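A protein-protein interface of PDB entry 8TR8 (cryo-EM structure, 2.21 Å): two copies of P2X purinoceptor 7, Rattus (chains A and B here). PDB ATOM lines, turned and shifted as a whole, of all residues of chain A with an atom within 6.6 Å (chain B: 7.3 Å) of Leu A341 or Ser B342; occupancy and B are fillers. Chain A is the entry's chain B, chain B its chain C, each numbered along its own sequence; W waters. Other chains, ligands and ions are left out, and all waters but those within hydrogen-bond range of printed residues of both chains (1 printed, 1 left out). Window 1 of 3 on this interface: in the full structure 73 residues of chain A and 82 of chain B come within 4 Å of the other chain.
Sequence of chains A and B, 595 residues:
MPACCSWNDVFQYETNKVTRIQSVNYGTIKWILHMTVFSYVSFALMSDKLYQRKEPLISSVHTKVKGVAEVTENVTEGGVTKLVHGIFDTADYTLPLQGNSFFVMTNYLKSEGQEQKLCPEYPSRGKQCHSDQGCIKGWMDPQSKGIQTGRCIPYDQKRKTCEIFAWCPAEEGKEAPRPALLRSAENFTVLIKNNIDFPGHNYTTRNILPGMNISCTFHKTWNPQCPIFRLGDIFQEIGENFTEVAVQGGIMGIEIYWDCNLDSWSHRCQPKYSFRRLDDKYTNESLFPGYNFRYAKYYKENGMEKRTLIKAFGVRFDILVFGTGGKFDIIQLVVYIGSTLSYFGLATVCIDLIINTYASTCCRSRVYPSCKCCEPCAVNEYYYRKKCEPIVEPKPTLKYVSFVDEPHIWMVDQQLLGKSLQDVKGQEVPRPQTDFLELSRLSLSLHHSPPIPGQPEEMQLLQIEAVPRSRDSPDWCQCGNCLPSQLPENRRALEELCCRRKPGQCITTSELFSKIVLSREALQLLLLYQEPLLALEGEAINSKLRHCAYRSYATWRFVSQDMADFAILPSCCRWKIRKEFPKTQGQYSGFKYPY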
ATOM      1  N   VAL A  37      -3.358  32.068   9.955  1.00  0.00           N
ATOM      2  CA  VAL A  37      -3.460  30.734  10.548  1.00  0.00           C
ATOM      3  C   VAL A  37      -3.930  30.831  11.991  1.00  0.00           C
ATOM      4  O   VAL A  37      -4.820  30.090  12.425  1.00  0.00           O
ATOM      5  CB  VAL A  37      -2.112  29.992  10.446  1.00  0.00           C
ATOM      6  CG1 VAL A  37      -2.138  28.705  11.266  1.00  0.00           C
ATOM      7  CG2 VAL A  37      -1.775  29.691   9.007  1.00  0.00           C
ATOM      8  N   TYR A 336      -6.051  19.248  19.983  1.00  0.00           N
ATOM      9  CA  TYR A 336      -6.393  20.219  18.947  1.00  0.00           C
ATOM     10  C   TYR A 336      -5.199  21.099  18.583  1.00  0.00           C
ATOM     11  O   TYR A 336      -4.922  21.328  17.398  1.00  0.00           O
ATOM     12  CB  TYR A 336      -7.568  21.086  19.392  1.00  0.00           C
ATOM     13  CG  TYR A 336      -7.882  22.181  18.412  1.00  0.00           C
ATOM     14  CD1 TYR A 336      -8.527  21.898  17.225  1.00  0.00           C
ATOM     15  CD2 TYR A 336      -7.509  23.491  18.656  1.00  0.00           C
ATOM     16  CE1 TYR A 336      -8.805  22.878  16.320  1.00  0.00           C
ATOM     17  CE2 TYR A 336      -7.783  24.481  17.754  1.00  0.00           C
ATOM     18  CZ  TYR A 336      -8.432  24.169  16.584  1.00  0.00           C
ATOM     19  OH  TYR A 336      -8.714  25.152  15.671  1.00  0.00           O
ATOM     20  N   ILE A 337      -4.486  21.605  19.590  1.00  0.00           N
ATOM     21  CA  ILE A 337      -3.330  22.458  19.326  1.00  0.00           C
ATOM     22  C   ILE A 337      -2.291  21.695  18.519  1.00  0.00           C
ATOM     23  O   ILE A 337      -1.706  22.228  17.570  1.00  0.00           O
ATOM     24  CB  ILE A 337      -2.742  22.996  20.642  1.00  0.00           C
ATOM     25  CG1 ILE A 337      -3.697  24.009  21.274  1.00  0.00           C
ATOM     26  CG2 ILE A 337      -1.371  23.621  20.403  1.00  0.00           C
ATOM     27  CD1 ILE A 337      -3.367  24.350  22.694  1.00  0.00           C
ATOM     28  N   GLY A 338      -2.040  20.439  18.888  1.00  0.00           N
ATOM     29  CA  GLY A 338      -1.104  19.634  18.129  1.00  0.00           C
ATOM     30  C   GLY A 338      -1.558  19.393  16.706  1.00  0.00           C
ATOM     31  O   GLY A 338      -0.751  19.407  15.774  1.00  0.00           O
ATOM     32  N   SER A 339      -2.858  19.156  16.517  1.00  0.00           N
ATOM     33  CA  SER A 339      -3.398  18.975  15.178  1.00  0.00           C
ATOM     34  C   SER A 339      -3.233  20.229  14.337  1.00  0.00           C
ATOM     35  O   SER A 339      -3.189  20.147  13.107  1.00  0.00           O
ATOM     36  CB  SER A 339      -4.875  18.593  15.259  1.00  0.00           C
ATOM     37  OG  SER A 339      -5.660  19.694  15.680  1.00  0.00           O
ATOM     38  N   THR A 340      -3.154  21.391  14.969  1.00  0.00           N
ATOM     39  CA  THR A 340      -3.076  22.631  14.211  1.00  0.00           C
ATOM     40  C   THR A 340      -1.667  23.208  14.115  1.00  0.00           C
ATOM     41  O   THR A 340      -1.452  24.143  13.336  1.00  0.00           O
ATOM     42  CB  THR A 340      -4.018  23.672  14.823  1.00  0.00           C
ATOM     43  OG1 THR A 340      -4.036  23.539  16.246  1.00  0.00           O
ATOM     44  CG2 THR A 340      -5.424  23.483  14.288  1.00  0.00           C
ATOM     45  N   LEU A 341      -0.704  22.668  14.863  1.00  0.00           N
ATOM     46  CA  LEU A 341       0.627  23.268  14.918  1.00  0.00           C
ATOM     47  C   LEU A 341       1.301  23.300  13.549  1.00  0.00           C
ATOM     48  O   LEU A 341       1.962  24.285  13.203  1.00  0.00           O
ATOM     49  CB  LEU A 341       1.496  22.507  15.916  1.00  0.00           C
ATOM     50  CG  LEU A 341       1.387  22.922  17.383  1.00  0.00           C
ATOM     51  CD1 LEU A 341       2.198  21.996  18.266  1.00  0.00           C
ATOM     52  CD2 LEU A 341       1.793  24.356  17.589  1.00  0.00           C
ATOM     53  N   SER A 342       1.166  22.230  12.767  1.00  0.00           N
ATOM     54  CA  SER A 342       1.858  22.154  11.486  1.00  0.00           C
ATOM     55  C   SER A 342       1.415  23.232  10.506  1.00  0.00           C
ATOM     56  O   SER A 342       2.154  23.534   9.565  1.00  0.00           O
ATOM     57  CB  SER A 342       1.648  20.780  10.857  1.00  0.00           C
ATOM     58  OG  SER A 342       2.541  19.834  11.394  1.00  0.00           O
ATOM     59  N   TYR A 343       0.233  23.817  10.693  1.00  0.00           N
ATOM     60  CA  TYR A 343      -0.247  24.838   9.774  1.00  0.00           C
ATOM     61  C   TYR A 343       0.567  26.123   9.849  1.00  0.00           C
ATOM     62  O   TYR A 343       0.426  26.976   8.969  1.00  0.00           O
ATOM     63  CB  TYR A 343      -1.724  25.135  10.043  1.00  0.00           C
ATOM     64  CG  TYR A 343      -2.672  24.153   9.402  1.00  0.00           C
ATOM     65  CD1 TYR A 343      -2.695  23.983   8.033  1.00  0.00           C
ATOM     66  CD2 TYR A 343      -3.549  23.399  10.168  1.00  0.00           C
ATOM     67  CE1 TYR A 343      -3.553  23.096   7.441  1.00  0.00           C
ATOM     68  CE2 TYR A 343      -4.412  22.509   9.583  1.00  0.00           C
ATOM     69  CZ  TYR A 343      -4.411  22.359   8.220  1.00  0.00           C
ATOM     70  OH  TYR A 343      -5.273  21.470   7.633  1.00  0.00           O
ATOM     71  N   PHE A 344       1.419  26.272  10.858  1.00  0.00           N
ATOM     72  CA  PHE A 344       2.268  27.444  10.990  1.00  0.00           C
ATOM     73  C   PHE A 344       3.540  27.361  10.150  1.00  0.00           C
ATOM     74  O   PHE A 344       4.324  28.313  10.149  1.00  0.00           O
ATOM     75  CB  PHE A 344       2.616  27.656  12.463  1.00  0.00           C
ATOM     76  CG  PHE A 344       1.467  28.157  13.283  1.00  0.00           C
ATOM     77  CD1 PHE A 344       1.130  29.497  13.282  1.00  0.00           C
ATOM     78  CD2 PHE A 344       0.710  27.286  14.046  1.00  0.00           C
ATOM     79  CE1 PHE A 344       0.069  29.954  14.027  1.00  0.00           C
ATOM     80  CE2 PHE A 344      -0.349  27.741  14.791  1.00  0.00           C
ATOM     81  CZ  PHE A 344      -0.671  29.076  14.781  1.00  0.00           C
ATOM     82  N   GLY A 345       3.767  26.250   9.451  1.00  0.00           N
ATOM     83  CA  GLY A 345       4.780  26.132   8.426  1.00  0.00           C
ATOM     84  C   GLY A 345       4.372  26.635   7.063  1.00  0.00           C
ATOM     85  O   GLY A 345       5.143  26.527   6.104  1.00  0.00           O
ATOM     86  N   VAL B  37       7.510  14.904  26.688  1.00  0.00           N
ATOM     87  CA  VAL B  37       6.476  14.851  25.658  1.00  0.00           C
ATOM     88  C   VAL B  37       6.003  13.418  25.458  1.00  0.00           C
ATOM     89  O   VAL B  37       4.798  13.146  25.383  1.00  0.00           O
ATOM     90  CB  VAL B  37       6.994  15.458  24.338  1.00  0.00           C
ATOM     91  CG1 VAL B  37       6.017  15.194  23.197  1.00  0.00           C
ATOM     92  CG2 VAL B  37       7.235  16.940  24.492  1.00  0.00           C
ATOM     93  N   ILE B 337      -1.505   9.887  16.834  1.00  0.00           N
ATOM     94  CA  ILE B 337      -0.053  10.009  16.740  1.00  0.00           C
ATOM     95  C   ILE B 337       0.316  11.212  15.887  1.00  0.00           C
ATOM     96  O   ILE B 337       1.227  11.977  16.227  1.00  0.00           O
ATOM     97  CB  ILE B 337       0.565   8.711  16.187  1.00  0.00           C
ATOM     98  CG1 ILE B 337       0.446   7.588  17.217  1.00  0.00           C
ATOM     99  CG2 ILE B 337       2.023   8.933  15.794  1.00  0.00           C
ATOM    100  CD1 ILE B 337       0.729   6.226  16.663  1.00  0.00           C
ATOM    101  N   GLY B 338      -0.375  11.394  14.763  1.00  0.00           N
ATOM    102  CA  GLY B 338      -0.115  12.552  13.932  1.00  0.00           C
ATOM    103  C   GLY B 338      -0.425  13.858  14.632  1.00  0.00           C
ATOM    104  O   GLY B 338       0.304  14.841  14.482  1.00  0.00           O
ATOM    105  N   SER B 339      -1.517  13.890  15.398  1.00  0.00           N
ATOM    106  CA  SER B 339      -1.859  15.081  16.160  1.00  0.00           C
ATOM    107  C   SER B 339      -0.798  15.403  17.197  1.00  0.00           C
ATOM    108  O   SER B 339      -0.657  16.560  17.601  1.00  0.00           O
ATOM    109  CB  SER B 339      -3.214  14.893  16.842  1.00  0.00           C
ATOM    110  OG  SER B 339      -3.120  13.958  17.901  1.00  0.00           O
ATOM    111  N   THR B 340      -0.055  14.405  17.651  1.00  0.00           N
ATOM    112  CA  THR B 340       0.923  14.640  18.704  1.00  0.00           C
ATOM    113  C   THR B 340       2.359  14.757  18.200  1.00  0.00           C
ATOM    114  O   THR B 340       3.236  15.151  18.973  1.00  0.00           O
ATOM    115  CB  THR B 340       0.834  13.526  19.753  1.00  0.00           C
ATOM    116  OG1 THR B 340       0.546  12.279  19.116  1.00  0.00           O
ATOM    117  CG2 THR B 340      -0.259  13.837  20.754  1.00  0.00           C
ATOM    118  N   LEU B 341       2.613  14.449  16.928  1.00  0.00           N
ATOM    119  CA  LEU B 341       3.987  14.405  16.429  1.00  0.00           C
ATOM    120  C   LEU B 341       4.686  15.756  16.552  1.00  0.00           C
ATOM    121  O   LEU B 341       5.870  15.816  16.897  1.00  0.00           O
ATOM    122  CB  LEU B 341       3.995  13.938  14.977  1.00  0.00           C
ATOM    123  CG  LEU B 341       3.996  12.427  14.738  1.00  0.00           C
ATOM    124  CD1 LEU B 341       3.866  12.116  13.260  1.00  0.00           C
ATOM    125  CD2 LEU B 341       5.216  11.771  15.323  1.00  0.00           C
ATOM    126  N   SER B 342       3.983  16.849  16.254  1.00  0.00           N
ATOM    127  CA  SER B 342       4.611  18.163  16.259  1.00  0.00           C
ATOM    128  C   SER B 342       5.125  18.570  17.633  1.00  0.00           C
ATOM    129  O   SER B 342       5.995  19.442  17.719  1.00  0.00           O
ATOM    130  CB  SER B 342       3.630  19.217  15.751  1.00  0.00           C
ATOM    131  OG  SER B 342       3.595  19.239  14.345  1.00  0.00           O
ATOM    132  N   TYR B 343       4.613  17.972  18.708  1.00  0.00           N
ATOM    133  CA  TYR B 343       5.055  18.340  20.044  1.00  0.00           C
ATOM    134  C   TYR B 343       6.496  17.929  20.321  1.00  0.00           C
ATOM    135  O   TYR B 343       7.070  18.384  21.313  1.00  0.00           O
ATOM    136  CB  TYR B 343       4.124  17.724  21.093  1.00  0.00           C
ATOM    137  CG  TYR B 343       2.860  18.511  21.326  1.00  0.00           C
ATOM    138  CD1 TYR B 343       2.910  19.816  21.771  1.00  0.00           C
ATOM    139  CD2 TYR B 343       1.612  17.944  21.105  1.00  0.00           C
ATOM    140  CE1 TYR B 343       1.768  20.539  21.986  1.00  0.00           C
ATOM    141  CE2 TYR B 343       0.462  18.662  21.319  1.00  0.00           C
ATOM    142  CZ  TYR B 343       0.544  19.957  21.760  1.00  0.00           C
ATOM    143  OH  TYR B 343      -0.603  20.674  21.974  1.00  0.00           O
ATOM    144  N   PHE B 344       7.091  17.105  19.465  1.00  0.00           N
ATOM    145  CA  PHE B 344       8.476  16.693  19.621  1.00  0.00           C
ATOM    146  C   PHE B 344       9.471  17.711  19.071  1.00  0.00           C
ATOM    147  O   PHE B 344      10.680  17.489  19.180  1.00  0.00           O
ATOM    148  CB  PHE B 344       8.680  15.333  18.952  1.00  0.00           C
ATOM    149  CG  PHE B 344       8.053  14.197  19.700  1.00  0.00           C
ATOM    150  CD1 PHE B 344       8.689  13.634  20.790  1.00  0.00           C
ATOM    151  CD2 PHE B 344       6.818  13.698  19.326  1.00  0.00           C
ATOM    152  CE1 PHE B 344       8.111  12.598  21.482  1.00  0.00           C
ATOM    153  CE2 PHE B 344       6.239  12.664  20.019  1.00  0.00           C
ATOM    154  CZ  PHE B 344       6.884  12.113  21.097  1.00  0.00           C
ATOM    155  N   GLY B 345       8.996  18.805  18.479  1.00  0.00           N
ATOM    156  CA  GLY B 345       9.801  19.960  18.146  1.00  0.00           C
ATOM    157  C   GLY B 345      10.012  20.936  19.276  1.00  0.00           C
ATOM    158  O   GLY B 345      10.636  21.986  19.082  1.00  0.00           O
ATOM    159  N   LEU B 346       9.492  20.613  20.461  1.00  0.00           N
ATOM    160  CA  LEU B 346       9.587  21.513  21.602  1.00  0.00           C
ATOM    161  C   LEU B 346      11.033  21.738  22.018  1.00  0.00           C
ATOM    162  O   LEU B 346      11.431  22.867  22.325  1.00  0.00           O
ATOM    163  CB  LEU B 346       8.774  20.950  22.767  1.00  0.00           C
ATOM    164  CG  LEU B 346       8.841  21.667  24.114  1.00  0.00           C
ATOM    165  CD1 LEU B 346       8.071  22.962  24.059  1.00  0.00           C
ATOM    166  CD2 LEU B 346       8.314  20.764  25.202  1.00  0.00           C
ATOM    167  N   VAL B 349      12.656  24.092  19.560  1.00  0.00           N
ATOM    168  CA  VAL B 349      12.167  25.456  19.736  1.00  0.00           C
ATOM    169  C   VAL B 349      12.830  26.104  20.947  1.00  0.00           C
ATOM    170  O   VAL B 349      13.345  27.227  20.870  1.00  0.00           O
ATOM    171  CB  VAL B 349      10.630  25.462  19.867  1.00  0.00           C
ATOM    172  CG1 VAL B 349      10.143  26.781  20.423  1.00  0.00           C
ATOM    173  CG2 VAL B 349       9.989  25.193  18.531  1.00  0.00           C
HETATM  174  O   HOH W   1       5.107  21.073  13.342  1.00  0.00           O
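The backbone NH (N) of Gly A338 sits at hydrogen-bond distance from the side-chain hydroxyl (OH) of Tyr B343, at 3.4 Å. The side-chain hydroxyl (OG) of Ser A342 lies within hydrogen-bond range of the side-chain hydroxyl (OG) of Ser B342 (3.2 Å). The backbone carbonyl oxygen of Gly A338 lies close to the backbone carbonyl oxygen of Ser B339, 3.4 Å away.
The side-chain hydroxyl of Ser A339 sits at hydrogen-bond distance from the backbone carbonyl oxygen of Tyr A336, at 2.5 Å. The side-chain hydroxyl (OG1) of Thr A340 lies within hydrogen-bond range of the backbone carbonyl oxygen (O) of Ile A337 (3.0 Å).
Among the printed residues, pairs that only touch across the chains: Ile A337 with Tyr B343 (3.4 Å), Ser A339 with Ser B339 (3.6 Å) and Leu A341 with Ser B342 (3.9 Å).
Of the printed residues of chain B, Leu A341 touches Ser B342. Of chain A, only Leu A341 and Ser A342 come within 4 Å of Ser B342. Of the printed residues of chain A, Tyr B343 touches Ile A337 and Gly A338. Printed residues of chain B within 4 Å of Ile A337: Tyr B343. Printed residues of chain B within 4 Å of Ser A342: Ser B342. Printed residues of chain B within 4 Å of Gly A338: Ser B339 (3.1 Å) and Tyr B343 (3.4 Å). Gly B345 touches none of the printed residues of chain A. Phe A344 touches none of the printed residues of chain B. The nearest residue of chain A that does not touch Ser B342 is Gly A338 (4.4 Å). The nearest printed residue of chain A that does not touch Tyr B343 is Leu A341 (4.02 Å).
Of the 12 printed residues of chain B, 3 touch a printed residue of chain A. Hydrophobic or aromatic side chains of chain B within 4 Å of the printed part of chain A: Tyr B343. Of the 11 printed residues of chain A, 5 touch a printed residue of chain B. Printed residues of chain A that touch a printed residue of chain B: Ile A337, Gly A338, Ser A339, Leu A341 and Ser A342. Hydrophobic or aromatic side chains of chain A within 4 Å of the printed part of chain B: Ile A337 and Leu A341. Among the printed residues, no Asp or Glu carboxylate lies within 4 Å of a Lys or Arg side-chain nitrogen of the other chain.
Gly A338 touches Ser B339, but with the chains exchanged Ser A339 does not touch Gly B338 (5.6 Å). Gly A338 touches Tyr B343, but with the chains exchanged Tyr A343 does not touch Gly B338 (9.7 Å). Ser A339 touches its own counterpart, Ser B339. Leu A341 touches Ser B342, but with the chains exchanged Ser A342 does not touch Leu B341 (6.9 Å). 10 positions are printed for both chains. Of the 6 pairs that touch across the chains among the printed residues, 2 have their exchanged pair printed and touching as well.
Water W1 bridges the side-chain hydroxyl of Ser B342 (2.6 Å) and the side-chain hydroxyl of Ser A342 (3.5 Å).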
